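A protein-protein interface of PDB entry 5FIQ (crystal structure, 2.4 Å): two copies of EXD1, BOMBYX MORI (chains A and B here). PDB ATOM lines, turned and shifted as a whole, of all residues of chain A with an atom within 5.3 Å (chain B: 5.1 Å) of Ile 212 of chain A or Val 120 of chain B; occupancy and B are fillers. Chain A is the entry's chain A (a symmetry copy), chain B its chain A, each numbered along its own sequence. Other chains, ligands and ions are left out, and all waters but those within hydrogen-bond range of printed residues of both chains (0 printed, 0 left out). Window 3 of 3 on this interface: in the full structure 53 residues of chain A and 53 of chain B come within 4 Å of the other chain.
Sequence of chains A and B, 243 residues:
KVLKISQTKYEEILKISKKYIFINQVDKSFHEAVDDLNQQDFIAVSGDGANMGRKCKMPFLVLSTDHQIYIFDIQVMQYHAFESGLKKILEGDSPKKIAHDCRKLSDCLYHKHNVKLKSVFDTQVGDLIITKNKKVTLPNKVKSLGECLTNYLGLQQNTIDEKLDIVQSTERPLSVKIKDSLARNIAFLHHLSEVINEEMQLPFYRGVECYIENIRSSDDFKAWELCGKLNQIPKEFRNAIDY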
ATOM      1  N   PHE A 204       4.881 -18.877  31.347  1.00  0.00           N
ATOM      2  CA  PHE A 204       5.306 -19.842  30.372  1.00  0.00           C
ATOM      3  C   PHE A 204       4.934 -21.260  30.683  1.00  0.00           C
ATOM      4  O   PHE A 204       4.294 -21.918  29.836  1.00  0.00           O
ATOM      5  CB  PHE A 204       6.804 -19.745  30.122  1.00  0.00           C
ATOM      6  CG  PHE A 204       7.346 -20.799  29.200  1.00  0.00           C
ATOM      7  CD1 PHE A 204       7.037 -20.764  27.857  1.00  0.00           C
ATOM      8  CD2 PHE A 204       8.155 -21.793  29.686  1.00  0.00           C
ATOM      9  CE1 PHE A 204       7.578 -21.675  27.022  1.00  0.00           C
ATOM     10  CE2 PHE A 204       8.704 -22.707  28.880  1.00  0.00           C
ATOM     11  CZ  PHE A 204       8.407 -22.667  27.526  1.00  0.00           C
ATOM     12  N   VAL A 208       2.236 -23.727  28.577  1.00  0.00           N
ATOM     13  CA  VAL A 208       2.577 -25.010  28.019  1.00  0.00           C
ATOM     14  C   VAL A 208       1.629 -26.050  28.519  1.00  0.00           C
ATOM     15  O   VAL A 208       1.213 -26.913  27.715  1.00  0.00           O
ATOM     16  CB  VAL A 208       4.016 -25.440  28.331  1.00  0.00           C
ATOM     17  CG1 VAL A 208       4.308 -26.886  27.927  1.00  0.00           C
ATOM     18  CG2 VAL A 208       4.986 -24.538  27.574  1.00  0.00           C
ATOM     19  N   GLU A 209       1.258 -25.987  29.792  1.00  0.00           N
ATOM     20  CA  GLU A 209       0.316 -26.947  30.300  1.00  0.00           C
ATOM     21  C   GLU A 209      -1.033 -26.777  29.635  1.00  0.00           C
ATOM     22  O   GLU A 209      -1.688 -27.746  29.425  1.00  0.00           O
ATOM     23  CB  GLU A 209       0.103 -26.862  31.805  1.00  0.00           C
ATOM     24  CG  GLU A 209       1.306 -27.317  32.618  1.00  0.00           C
ATOM     25  CD  GLU A 209       1.381 -26.661  34.055  1.00  0.00           C
ATOM     26  OE1 GLU A 209       0.275 -26.373  34.675  1.00  0.00           O
ATOM     27  OE2 GLU A 209       2.537 -26.472  34.586  1.00  0.00           O
ATOM     28  N   CYS A 210      -1.446 -25.549  29.403  1.00  0.00           N
ATOM     29  CA  CYS A 210      -2.679 -25.294  28.754  1.00  0.00           C
ATOM     30  C   CYS A 210      -2.646 -26.000  27.310  1.00  0.00           C
ATOM     31  O   CYS A 210      -3.532 -26.774  27.032  1.00  0.00           O
ATOM     32  CB  CYS A 210      -2.874 -23.809  28.636  1.00  0.00           C
ATOM     33  SG  CYS A 210      -4.293 -23.406  27.625  1.00  0.00           S
ATOM     34  N   TYR A 211      -1.571 -25.810  26.528  1.00  0.00           N
ATOM     35  CA  TYR A 211      -1.361 -26.529  25.290  1.00  0.00           C
ATOM     36  C   TYR A 211      -1.439 -28.053  25.334  1.00  0.00           C
ATOM     37  O   TYR A 211      -2.144 -28.681  24.541  1.00  0.00           O
ATOM     38  CB  TYR A 211      -0.007 -26.151  24.707  1.00  0.00           C
ATOM     39  CG  TYR A 211      -0.075 -25.050  23.679  1.00  0.00           C
ATOM     40  CD1 TYR A 211      -0.636 -23.846  23.989  1.00  0.00           C
ATOM     41  CD2 TYR A 211       0.486 -25.213  22.387  1.00  0.00           C
ATOM     42  CE1 TYR A 211      -0.674 -22.812  23.051  1.00  0.00           C
ATOM     43  CE2 TYR A 211       0.442 -24.207  21.471  1.00  0.00           C
ATOM     44  CZ  TYR A 211      -0.129 -23.018  21.806  1.00  0.00           C
ATOM     45  OH  TYR A 211      -0.189 -22.014  20.899  1.00  0.00           O
ATOM     46  N   ILE A 212      -0.676 -28.642  26.244  1.00  0.00           N
ATOM     47  CA  ILE A 212      -0.782 -30.093  26.490  1.00  0.00           C
ATOM     48  C   ILE A 212      -2.218 -30.592  26.818  1.00  0.00           C
ATOM     49  O   ILE A 212      -2.573 -31.704  26.450  1.00  0.00           O
ATOM     50  CB  ILE A 212       0.088 -30.536  27.653  1.00  0.00           C
ATOM     51  CG1 ILE A 212       1.561 -30.342  27.320  1.00  0.00           C
ATOM     52  CG2 ILE A 212      -0.160 -31.977  28.047  1.00  0.00           C
ATOM     53  CD1 ILE A 212       2.511 -30.583  28.502  1.00  0.00           C
ATOM     54  N   GLU A 213      -3.041 -29.783  27.446  1.00  0.00           N
ATOM     55  CA  GLU A 213      -4.408 -30.211  27.795  1.00  0.00           C
ATOM     56  C   GLU A 213      -5.481 -29.880  26.758  1.00  0.00           C
ATOM     57  O   GLU A 213      -6.543 -30.502  26.749  1.00  0.00           O
ATOM     58  CB  GLU A 213      -4.872 -29.571  29.160  1.00  0.00           C
ATOM     59  CG  GLU A 213      -4.389 -30.220  30.452  1.00  0.00           C
ATOM     60  CD  GLU A 213      -4.327 -31.768  30.461  1.00  0.00           C
ATOM     61  OE1 GLU A 213      -5.251 -32.489  29.916  1.00  0.00           O
ATOM     62  OE2 GLU A 213      -3.310 -32.274  31.031  1.00  0.00           O
ATOM     63  N   ASN A 214      -5.245 -28.813  26.015  1.00  0.00           N
ATOM     64  CA  ASN A 214      -6.282 -28.101  25.262  1.00  0.00           C
ATOM     65  C   ASN A 214      -7.056 -29.041  24.349  1.00  0.00           C
ATOM     66  O   ASN A 214      -8.284 -29.070  24.385  1.00  0.00           O
ATOM     67  CB  ASN A 214      -5.619 -27.042  24.397  1.00  0.00           C
ATOM     68  CG  ASN A 214      -6.601 -26.265  23.542  1.00  0.00           C
ATOM     69  OD1 ASN A 214      -7.450 -25.561  24.048  1.00  0.00           O
ATOM     70  ND2 ASN A 214      -6.475 -26.377  22.219  1.00  0.00           N
ATOM     71  N   ILE A 215      -6.352 -29.872  23.608  1.00  0.00           N
ATOM     72  CA  ILE A 215      -7.036 -30.824  22.734  1.00  0.00           C
ATOM     73  C   ILE A 215      -7.236 -32.168  23.455  1.00  0.00           C
ATOM     74  O   ILE A 215      -8.322 -32.750  23.412  1.00  0.00           O
ATOM     75  CB  ILE A 215      -6.289 -30.949  21.352  1.00  0.00           C
ATOM     76  CG1 ILE A 215      -6.163 -29.561  20.755  1.00  0.00           C
ATOM     77  CG2 ILE A 215      -7.001 -31.888  20.434  1.00  0.00           C
ATOM     78  CD1 ILE A 215      -5.737 -29.502  19.338  1.00  0.00           C
ATOM     79  N   ARG A 216      -6.173 -32.681  24.031  1.00  0.00           N
ATOM     80  CA  ARG A 216      -6.162 -33.969  24.694  1.00  0.00           C
ATOM     81  C   ARG A 216      -7.328 -34.172  25.681  1.00  0.00           C
ATOM     82  O   ARG A 216      -7.817 -35.288  25.818  1.00  0.00           O
ATOM     83  CB  ARG A 216      -4.819 -34.149  25.393  1.00  0.00           C
ATOM     84  CG  ARG A 216      -4.641 -35.486  26.065  1.00  0.00           C
ATOM     85  CD  ARG A 216      -4.066 -35.235  27.437  1.00  0.00           C
ATOM     86  NE  ARG A 216      -2.644 -35.419  27.429  1.00  0.00           N
ATOM     87  CZ  ARG A 216      -1.797 -34.983  28.326  1.00  0.00           C
ATOM     88  NH1 ARG A 216      -2.166 -34.202  29.332  1.00  0.00           N
ATOM     89  NH2 ARG A 216      -0.527 -35.304  28.159  1.00  0.00           N
ATOM     90  N   LYS B  96      13.045 -33.020  29.456  1.00  0.00           N
ATOM     91  CA  LYS B  96      12.049 -32.063  28.900  1.00  0.00           C
ATOM     92  C   LYS B  96      11.988 -32.337  27.432  1.00  0.00           C
ATOM     93  O   LYS B  96      13.027 -32.490  26.807  1.00  0.00           O
ATOM     94  CB  LYS B  96      12.400 -30.549  29.068  1.00  0.00           C
ATOM     95  CG  LYS B  96      12.205 -30.038  30.458  1.00  0.00           C
ATOM     96  CD  LYS B  96      11.973 -28.499  30.579  1.00  0.00           C
ATOM     97  CE  LYS B  96      10.507 -28.141  30.624  1.00  0.00           C
ATOM     98  NZ  LYS B  96       9.929 -28.587  31.940  1.00  0.00           N
ATOM     99  N   LYS B  97      10.810 -32.291  26.882  1.00  0.00           N
ATOM    100  CA  LYS B  97      10.603 -32.451  25.389  1.00  0.00           C
ATOM    101  C   LYS B  97      10.418 -31.092  24.831  1.00  0.00           C
ATOM    102  O   LYS B  97       9.519 -30.350  25.209  1.00  0.00           O
ATOM    103  CB  LYS B  97       9.361 -33.272  25.078  1.00  0.00           C
ATOM    104  CG  LYS B  97       9.606 -34.765  25.094  1.00  0.00           C
ATOM    105  CD  LYS B  97       9.943 -35.359  26.465  1.00  0.00           C
ATOM    106  CE  LYS B  97       8.909 -35.025  27.530  1.00  0.00           C
ATOM    107  NZ  LYS B  97       8.988 -35.893  28.717  1.00  0.00           N
ATOM    108  N   ALA B  99       9.143 -29.014  21.802  1.00  0.00           N
ATOM    109  CA  ALA B  99       8.179 -29.165  20.740  1.00  0.00           C
ATOM    110  C   ALA B  99       7.695 -27.810  20.265  1.00  0.00           C
ATOM    111  O   ALA B  99       7.763 -26.837  21.040  1.00  0.00           O
ATOM    112  CB  ALA B  99       6.991 -29.973  21.194  1.00  0.00           C
ATOM    113  N   CYS B 102       2.503 -28.429  20.630  1.00  0.00           N
ATOM    114  CA  CYS B 102       2.356 -29.800  20.910  1.00  0.00           C
ATOM    115  C   CYS B 102       0.914 -30.161  21.074  1.00  0.00           C
ATOM    116  O   CYS B 102       0.623 -31.280  21.517  1.00  0.00           O
ATOM    117  CB  CYS B 102       3.094 -30.089  22.193  1.00  0.00           C
ATOM    118  SG  CYS B 102       2.400 -29.273  23.691  1.00  0.00           S
ATOM    119  N   SER B 106      -0.026 -34.042  21.772  1.00  0.00           N
ATOM    120  CA  SER B 106      -0.536 -34.449  23.067  1.00  0.00           C
ATOM    121  C   SER B 106      -1.755 -35.292  22.841  1.00  0.00           C
ATOM    122  O   SER B 106      -1.833 -36.417  23.309  1.00  0.00           O
ATOM    123  CB  SER B 106      -0.894 -33.230  23.956  1.00  0.00           C
ATOM    124  OG  SER B 106      -1.290 -33.633  25.263  1.00  0.00           O
ATOM    125  N   LEU B 117       1.771 -37.293  27.471  1.00  0.00           N
ATOM    126  CA  LEU B 117       2.914 -36.410  27.248  1.00  0.00           C
ATOM    127  C   LEU B 117       3.037 -35.452  28.440  1.00  0.00           C
ATOM    128  O   LEU B 117       2.084 -34.870  28.850  1.00  0.00           O
ATOM    129  CB  LEU B 117       2.703 -35.612  25.979  1.00  0.00           C
ATOM    130  CG  LEU B 117       3.777 -34.613  25.589  1.00  0.00           C
ATOM    131  CD1 LEU B 117       5.075 -35.346  25.225  1.00  0.00           C
ATOM    132  CD2 LEU B 117       3.382 -33.735  24.421  1.00  0.00           C
ATOM    133  N   LYS B 118       4.233 -35.274  28.942  1.00  0.00           N
ATOM    134  CA  LYS B 118       4.445 -34.345  30.015  1.00  0.00           C
ATOM    135  C   LYS B 118       5.839 -33.770  29.998  1.00  0.00           C
ATOM    136  O   LYS B 118       6.758 -34.393  29.488  1.00  0.00           O
ATOM    137  CB  LYS B 118       4.250 -35.069  31.321  1.00  0.00           C
ATOM    138  CG  LYS B 118       4.124 -34.116  32.469  1.00  0.00           C
ATOM    139  CD  LYS B 118       3.680 -34.789  33.743  1.00  0.00           C
ATOM    140  CE  LYS B 118       4.811 -34.828  34.696  1.00  0.00           C
ATOM    141  NZ  LYS B 118       4.475 -34.703  36.153  1.00  0.00           N
ATOM    142  N   SER B 119       5.969 -32.578  30.571  1.00  0.00           N
ATOM    143  CA  SER B 119       7.223 -31.814  30.719  1.00  0.00           C
ATOM    144  C   SER B 119       7.754 -31.345  29.352  1.00  0.00           C
ATOM    145  O   SER B 119       8.594 -31.992  28.756  1.00  0.00           O
ATOM    146  CB  SER B 119       8.279 -32.625  31.452  1.00  0.00           C
ATOM    147  OG  SER B 119       9.336 -31.773  31.759  1.00  0.00           O
ATOM    148  N   VAL B 120       7.302 -30.184  28.929  1.00  0.00           N
ATOM    149  CA  VAL B 120       7.514 -29.745  27.601  1.00  0.00           C
ATOM    150  C   VAL B 120       7.978 -28.316  27.558  1.00  0.00           C
ATOM    151  O   VAL B 120       7.446 -27.506  28.239  1.00  0.00           O
ATOM    152  CB  VAL B 120       6.210 -29.891  26.788  1.00  0.00           C
ATOM    153  CG1 VAL B 120       6.284 -29.251  25.413  1.00  0.00           C
ATOM    154  CG2 VAL B 120       5.866 -31.373  26.626  1.00  0.00           C
ATOM    155  N   PHE B 121       8.885 -28.018  26.630  1.00  0.00           N
ATOM    156  CA  PHE B 121       9.260 -26.600  26.377  1.00  0.00           C
ATOM    157  C   PHE B 121       8.719 -26.362  24.964  1.00  0.00           C
ATOM    158  O   PHE B 121       9.227 -26.926  24.023  1.00  0.00           O
ATOM    159  CB  PHE B 121      10.778 -26.427  26.449  1.00  0.00           C
ATOM    160  CG  PHE B 121      11.226 -25.043  26.218  1.00  0.00           C
ATOM    161  CD1 PHE B 121      11.155 -24.447  24.975  1.00  0.00           C
ATOM    162  CD2 PHE B 121      11.732 -24.289  27.306  1.00  0.00           C
ATOM    163  CE1 PHE B 121      11.614 -23.147  24.748  1.00  0.00           C
ATOM    164  CE2 PHE B 121      12.142 -22.992  27.126  1.00  0.00           C
ATOM    165  CZ  PHE B 121      12.092 -22.418  25.816  1.00  0.00           C
ATOM    166  N   ASP B 122       7.660 -25.582  24.844  1.00  0.00           N
ATOM    167  CA  ASP B 122       6.911 -25.447  23.620  1.00  0.00           C
ATOM    168  C   ASP B 122       7.292 -24.110  23.034  1.00  0.00           C
ATOM    169  O   ASP B 122       6.937 -23.067  23.636  1.00  0.00           O
ATOM    170  CB  ASP B 122       5.388 -25.538  23.845  1.00  0.00           C
ATOM    171  CG  ASP B 122       4.616 -25.735  22.563  1.00  0.00           C
ATOM    172  OD1 ASP B 122       4.838 -24.863  21.679  1.00  0.00           O
ATOM    173  OD2 ASP B 122       3.796 -26.702  22.458  1.00  0.00           O
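No position is printed for both chains.
Of the 11 pairs that touch across the chains among the printed residues, none has its exchanged pair printed and touching as well.
Of the printed residues of chain B, Ile 212 of chain A touches Cys 102 (3.9 Å), Ser 106 (2.6 Å), Leu 117 (3.7 Å) and Val 120 (3.9 Å).
Of chain A, only Val 208 (3.2 Å) and Ile 212 (3.9 Å) come within 4 Å of Val 120 of chain B.
Printed residues of chain A within 4 Å of Phe 121 of chain B: Phe 204 (3.7 Å).
Of the printed residues of chain B, Tyr 211 of chain A touches Asp 122 (3.6 Å).
Printed residues of chain B within 4 Å of Phe 204 of chain A: Phe 121 (3.7 Å) and Asp 122 (3.7 Å).
Printed residues of chain A within 4 Å of Ser 106 of chain B: Ile 212 and Arg 216.
The nearest printed residue of chain B that does not touch Phe 204 of chain A is Val 120 of chain B (5.0 Å).
The side-chain hydroxyl (OG) of Ser 106 of chain B lies within hydrogen-bond range of the guanidinium group (NE) of Arg 216 of chain A (3.1 Å).
The guanidinium group (NH2) of Arg 216 of chain A sits at hydrogen-bond distance from the backbone carbonyl oxygen (O) of Leu 117 of chain B, 2.7 Å away.
The side-chain hydroxyl of Ser 106 of chain B sits at hydrogen-bond distance from the backbone carbonyl oxygen of Ile 212 of chain A, 2.6 Å away.
Of the 11 printed residues of chain B, 6 touch a printed residue of chain A.
Hydrophobic or aromatic side chains of chain B within 4 Å of the printed part of chain A: Leu 117, Val 120 and Phe 121.
Along chain A the printed residues that touch a printed residue of chain B span positions 204 to 216.
Among the printed residues, 11 pairs touch across the chains.
Among the printed residues, no Asp or Glu carboxylate lies within 4 Å of a Lys or Arg side-chain nitrogen of the other chain.
Among the printed residues, merely in contact across the chains: Phe 204 of chain A with Phe 121 of chain B (3.7 Å), Phe 204 of chain A with Asp 122 of chain B (3.7 Å), Val 208 of chain A with Val 120 of chain B (3.2 Å), Val 208 of chain A with Asp 122 of chain B (3.9 Å), Tyr 211 of chain A with Asp 122 of chain B (3.6 Å), Ile 212 of chain A with Cys 102 of chain B (3.9 Å), Ile 212 of chain A with Leu 117 of chain B (3.7 Å) and Ile 212 of chain A with Val 120 of chain B (3.9 Å).
The backbone NH of Phe 121 of chain B sits at hydrogen-bond distance from the backbone carbonyl oxygen of Lys 97 of chain B (2.8 Å).
N of Ala 99 of chain B lies within hydrogen-bond range of O of Phe 121 of chain B, 3.0 Å away.
The side-chain carboxylate (OE2) of Glu 213 of chain A lies within salt-bridge range of the guanidinium group (NH1) of Arg 216 of chain A (2.8 Å).
The side-chain carboxylate (OD2) of Asp 122 of chain B sits at hydrogen-bond distance from the backbone NH (N) of Cys 102 of chain B (2.8 Å).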
